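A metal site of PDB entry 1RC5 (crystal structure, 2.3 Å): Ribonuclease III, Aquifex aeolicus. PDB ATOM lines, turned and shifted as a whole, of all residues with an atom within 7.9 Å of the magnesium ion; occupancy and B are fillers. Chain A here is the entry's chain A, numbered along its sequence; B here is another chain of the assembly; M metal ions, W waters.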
ATOM      1  N   TYR A  37       1.878   2.290  12.256  1.00  0.00           N
ATOM      2  CA  TYR A  37       1.375   2.072  13.604  1.00  0.00           C
ATOM      3  C   TYR A  37       2.066   2.917  14.670  1.00  0.00           C
ATOM      4  O   TYR A  37       1.631   2.826  15.829  1.00  0.00           O
ATOM      5  CB  TYR A  37       1.480   0.597  13.995  1.00  0.00           C
ATOM      6  CG  TYR A  37       2.797  -0.110  14.156  1.00  0.00           C
ATOM      7  CD1 TYR A  37       3.643   0.090  15.236  1.00  0.00           C
ATOM      8  CD2 TYR A  37       3.243  -1.034  13.206  1.00  0.00           C
ATOM      9  CE1 TYR A  37       4.855  -0.542  15.386  1.00  0.00           C
ATOM     10  CE2 TYR A  37       4.459  -1.691  13.353  1.00  0.00           C
ATOM     11  CZ  TYR A  37       5.263  -1.448  14.436  1.00  0.00           C
ATOM     12  OH  TYR A  37       6.467  -2.080  14.607  1.00  0.00           O
ATOM     13  N   GLU A  38       3.102   3.678  14.375  1.00  0.00           N
ATOM     14  CA  GLU A  38       3.926   4.259  15.439  1.00  0.00           C
ATOM     15  C   GLU A  38       3.165   5.065  16.483  1.00  0.00           C
ATOM     16  O   GLU A  38       3.494   4.984  17.671  1.00  0.00           O
ATOM     17  CB  GLU A  38       5.020   5.164  14.857  1.00  0.00           C
ATOM     18  CG  GLU A  38       6.069   5.575  15.891  1.00  0.00           C
ATOM     19  CD  GLU A  38       6.897   6.758  15.434  1.00  0.00           C
ATOM     20  OE1 GLU A  38       7.750   6.571  14.534  1.00  0.00           O
ATOM     21  OE2 GLU A  38       6.716   7.867  15.968  1.00  0.00           O
ATOM     22  N   GLU A  41       0.702   2.898  18.550  1.00  0.00           N
ATOM     23  CA  GLU A  41       1.531   2.175  19.498  1.00  0.00           C
ATOM     24  C   GLU A  41       1.810   3.040  20.718  1.00  0.00           C
ATOM     25  O   GLU A  41       1.895   2.548  21.850  1.00  0.00           O
ATOM     26  CB  GLU A  41       2.863   1.741  18.893  1.00  0.00           C
ATOM     27  CG  GLU A  41       3.653   0.856  19.857  1.00  0.00           C
ATOM     28  CD  GLU A  41       5.140   0.839  19.590  1.00  0.00           C
ATOM     29  OE1 GLU A  41       5.593   1.457  18.604  1.00  0.00           O
ATOM     30  OE2 GLU A  41       5.863   0.208  20.394  1.00  0.00           O
ATOM     31  N   PHE A  42       1.963   4.349  20.485  1.00  0.00           N
ATOM     32  CA  PHE A  42       2.224   5.210  21.633  1.00  0.00           C
ATOM     33  C   PHE A  42       1.048   5.129  22.609  1.00  0.00           C
ATOM     34  O   PHE A  42       1.215   4.890  23.808  1.00  0.00           O
ATOM     35  CB  PHE A  42       2.486   6.651  21.191  1.00  0.00           C
ATOM     36  CG  PHE A  42       3.341   7.428  22.179  1.00  0.00           C
ATOM     37  CD1 PHE A  42       4.647   7.025  22.444  1.00  0.00           C
ATOM     38  CD2 PHE A  42       2.837   8.531  22.833  1.00  0.00           C
ATOM     39  CE1 PHE A  42       5.432   7.724  23.349  1.00  0.00           C
ATOM     40  CE2 PHE A  42       3.610   9.236  23.737  1.00  0.00           C
ATOM     41  CZ  PHE A  42       4.909   8.837  23.996  1.00  0.00           C
ATOM     42  N   GLY A  44      -1.686   2.912  22.749  1.00  0.00           N
ATOM     43  CA  GLY A  44      -1.965   1.566  23.214  1.00  0.00           C
ATOM     44  C   GLY A  44      -1.006   1.099  24.289  1.00  0.00           C
ATOM     45  O   GLY A  44      -1.350   0.269  25.136  1.00  0.00           O
ATOM     46  N   ASP A  45       0.208   1.624  24.283  1.00  0.00           N
ATOM     47  CA  ASP A  45       1.147   1.312  25.360  1.00  0.00           C
ATOM     48  C   ASP A  45       0.549   1.733  26.697  1.00  0.00           C
ATOM     49  O   ASP A  45       0.415   0.947  27.629  1.00  0.00           O
ATOM     50  CB  ASP A  45       2.488   1.991  25.085  1.00  0.00           C
ATOM     51  CG  ASP A  45       3.580   1.705  26.087  1.00  0.00           C
ATOM     52  OD1 ASP A  45       3.274   1.460  27.263  1.00  0.00           O
ATOM     53  OD2 ASP A  45       4.774   1.733  25.697  1.00  0.00           O
ATOM     54  N   GLU A  78       7.397  -8.052  26.475  1.00  0.00           N
ATOM     55  CA  GLU A  78       7.054  -8.293  25.065  1.00  0.00           C
ATOM     56  C   GLU A  78       6.843  -9.782  24.848  1.00  0.00           C
ATOM     57  O   GLU A  78       6.253 -10.217  23.861  1.00  0.00           O
ATOM     58  CB  GLU A  78       8.136  -7.770  24.126  1.00  0.00           C
ATOM     59  CG  GLU A  78       8.472  -8.741  23.002  1.00  0.00           C
ATOM     60  CD  GLU A  78       9.825  -8.393  22.405  1.00  0.00           C
ATOM     61  OE1 GLU A  78      10.154  -7.196  22.461  1.00  0.00           O
ATOM     62  OE2 GLU A  78      10.510  -9.301  21.903  1.00  0.00           O
ATOM     63  N   PHE A  81       3.218 -10.200  25.915  1.00  0.00           N
ATOM     64  CA  PHE A  81       2.358  -9.577  24.911  1.00  0.00           C
ATOM     65  C   PHE A  81       2.238 -10.485  23.687  1.00  0.00           C
ATOM     66  O   PHE A  81       1.196 -10.526  23.036  1.00  0.00           O
ATOM     67  CB  PHE A  81       2.863  -8.201  24.496  1.00  0.00           C
ATOM     68  CG  PHE A  81       2.355  -7.043  25.340  1.00  0.00           C
ATOM     69  CD1 PHE A  81       1.751  -7.275  26.569  1.00  0.00           C
ATOM     70  CD2 PHE A  81       2.481  -5.739  24.899  1.00  0.00           C
ATOM     71  CE1 PHE A  81       1.288  -6.219  27.347  1.00  0.00           C
ATOM     72  CE2 PHE A  81       2.046  -4.674  25.673  1.00  0.00           C
ATOM     73  CZ  PHE A  81       1.450  -4.920  26.900  1.00  0.00           C
ATOM     74  N   THR A 104       9.022  -8.275  18.856  1.00  0.00           N
ATOM     75  CA  THR A 104       8.989  -6.870  19.238  1.00  0.00           C
ATOM     76  C   THR A 104       7.964  -6.101  18.399  1.00  0.00           C
ATOM     77  O   THR A 104       7.156  -5.339  18.930  1.00  0.00           O
ATOM     78  CB  THR A 104      10.352  -6.179  19.050  1.00  0.00           C
ATOM     79  OG1 THR A 104      11.327  -6.709  19.948  1.00  0.00           O
ATOM     80  CG2 THR A 104      10.216  -4.695  19.378  1.00  0.00           C
ATOM     81  N   ILE A 105       8.012  -6.296  17.091  1.00  0.00           N
ATOM     82  CA  ILE A 105       7.127  -5.625  16.148  1.00  0.00           C
ATOM     83  C   ILE A 105       5.681  -6.048  16.383  1.00  0.00           C
ATOM     84  O   ILE A 105       4.758  -5.255  16.256  1.00  0.00           O
ATOM     85  CB  ILE A 105       7.579  -5.941  14.710  1.00  0.00           C
ATOM     86  CG1 ILE A 105       8.842  -5.193  14.281  1.00  0.00           C
ATOM     87  CG2 ILE A 105       6.448  -5.703  13.715  1.00  0.00           C
ATOM     88  CD1 ILE A 105       9.201  -5.440  12.832  1.00  0.00           C
ATOM     89  N   GLY A 107       4.592  -7.121  19.304  1.00  0.00           N
ATOM     90  CA  GLY A 107       4.202  -6.476  20.554  1.00  0.00           C
ATOM     91  C   GLY A 107       3.807  -5.036  20.296  1.00  0.00           C
ATOM     92  O   GLY A 107       2.855  -4.527  20.899  1.00  0.00           O
ATOM     93  N   ASP A 108       4.519  -4.352  19.393  1.00  0.00           N
ATOM     94  CA  ASP A 108       4.207  -2.966  19.076  1.00  0.00           C
ATOM     95  C   ASP A 108       2.866  -2.811  18.361  1.00  0.00           C
ATOM     96  O   ASP A 108       2.183  -1.797  18.477  1.00  0.00           O
ATOM     97  CB  ASP A 108       5.308  -2.370  18.189  1.00  0.00           C
ATOM     98  CG  ASP A 108       6.609  -2.232  18.941  1.00  0.00           C
ATOM     99  OD1 ASP A 108       6.541  -2.176  20.191  1.00  0.00           O
ATOM    100  OD2 ASP A 108       7.683  -2.190  18.291  1.00  0.00           O
ATOM    101  N   VAL A 109       2.507  -3.833  17.598  1.00  0.00           N
ATOM    102  CA  VAL A 109       1.269  -3.888  16.836  1.00  0.00           C
ATOM    103  C   VAL A 109       0.123  -4.267  17.766  1.00  0.00           C
ATOM    104  O   VAL A 109      -1.017  -3.814  17.614  1.00  0.00           O
ATOM    105  CB  VAL A 109       1.401  -4.878  15.665  1.00  0.00           C
ATOM    106  CG1 VAL A 109       0.066  -5.156  14.995  1.00  0.00           C
ATOM    107  CG2 VAL A 109       2.397  -4.338  14.653  1.00  0.00           C
ATOM    108  N   PHE A 110       0.462  -5.096  18.752  1.00  0.00           N
ATOM    109  CA  PHE A 110      -0.526  -5.472  19.761  1.00  0.00           C
ATOM    110  C   PHE A 110      -1.003  -4.182  20.423  1.00  0.00           C
ATOM    111  O   PHE A 110      -2.198  -3.912  20.504  1.00  0.00           O
ATOM    112  CB  PHE A 110       0.050  -6.462  20.768  1.00  0.00           C
ATOM    113  CG  PHE A 110      -0.979  -7.055  21.709  1.00  0.00           C
ATOM    114  CD1 PHE A 110      -1.918  -7.965  21.265  1.00  0.00           C
ATOM    115  CD2 PHE A 110      -1.010  -6.694  23.050  1.00  0.00           C
ATOM    116  CE1 PHE A 110      -2.857  -8.500  22.117  1.00  0.00           C
ATOM    117  CE2 PHE A 110      -1.944  -7.234  23.923  1.00  0.00           C
ATOM    118  CZ  PHE A 110      -2.862  -8.151  23.458  1.00  0.00           C
ATOM    119  N   GLU A 111      -0.046  -3.381  20.862  1.00  0.00           N
ATOM    120  CA  GLU A 111      -0.369  -2.078  21.454  1.00  0.00           C
ATOM    121  C   GLU A 111      -1.223  -1.261  20.479  1.00  0.00           C
ATOM    122  O   GLU A 111      -2.282  -0.758  20.841  1.00  0.00           O
ATOM    123  CB  GLU A 111       0.899  -1.330  21.852  1.00  0.00           C
ATOM    124  CG  GLU A 111       1.747  -2.063  22.893  1.00  0.00           C
ATOM    125  CD  GLU A 111       3.081  -1.439  23.224  1.00  0.00           C
ATOM    126  OE1 GLU A 111       3.670  -0.736  22.367  1.00  0.00           O
ATOM    127  OE2 GLU A 111       3.583  -1.616  24.352  1.00  0.00           O
ATOM    128  N   ALA A 112      -0.768  -1.145  19.231  1.00  0.00           N
ATOM    129  CA  ALA A 112      -1.416  -0.291  18.241  1.00  0.00           C
ATOM    130  C   ALA A 112      -2.848  -0.726  17.927  1.00  0.00           C
ATOM    131  O   ALA A 112      -3.719   0.080  17.605  1.00  0.00           O
ATOM    132  CB  ALA A 112      -0.587  -0.261  16.966  1.00  0.00           C
ATOM    133  N   GLU B  65       7.158   9.393  17.938  1.00  0.00           N
ATOM    134  CA  GLU B  65       7.473   9.016  19.306  1.00  0.00           C
ATOM    135  C   GLU B  65       8.633   9.814  19.883  1.00  0.00           C
ATOM    136  O   GLU B  65       8.686  10.074  21.097  1.00  0.00           O
ATOM    137  CB  GLU B  65       7.799   7.531  19.400  1.00  0.00           C
ATOM    138  CG  GLU B  65       7.470   6.906  20.747  1.00  0.00           C
ATOM    139  CD  GLU B  65       8.679   6.294  21.426  1.00  0.00           C
ATOM    140  OE1 GLU B  65       9.818   6.650  21.034  1.00  0.00           O
ATOM    141  OE2 GLU B  65       8.494   5.469  22.338  1.00  0.00           O
HETATM  142 MG    MG M   1       5.880  -0.681  22.156  1.00  0.00          MG
HETATM  143  O   HOH W   1       6.656  -1.704  23.788  1.00  0.00           O
HETATM  144  O   HOH W   2       8.127   0.001  22.385  1.00  0.00           O
HETATM  145  O   HOH W   3       5.685   1.469  23.559  1.00  0.00           O
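Three residues have an atom within 4 Å of the magnesium ion: Glu 41, Asp 108 and Glu 111.
The magnesium ion is bound by the side-chain carboxylate (OE2) of Glu 41 (2.0 Å), water W1 (2.1 Å), the side-chain carboxylate (OE1) of Glu 111 (2.2 Å), water W2 (2.4 Å), the side-chain carboxylate (OD1) of Asp 108 (2.6 Å) and water W3 (2.6 Å).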
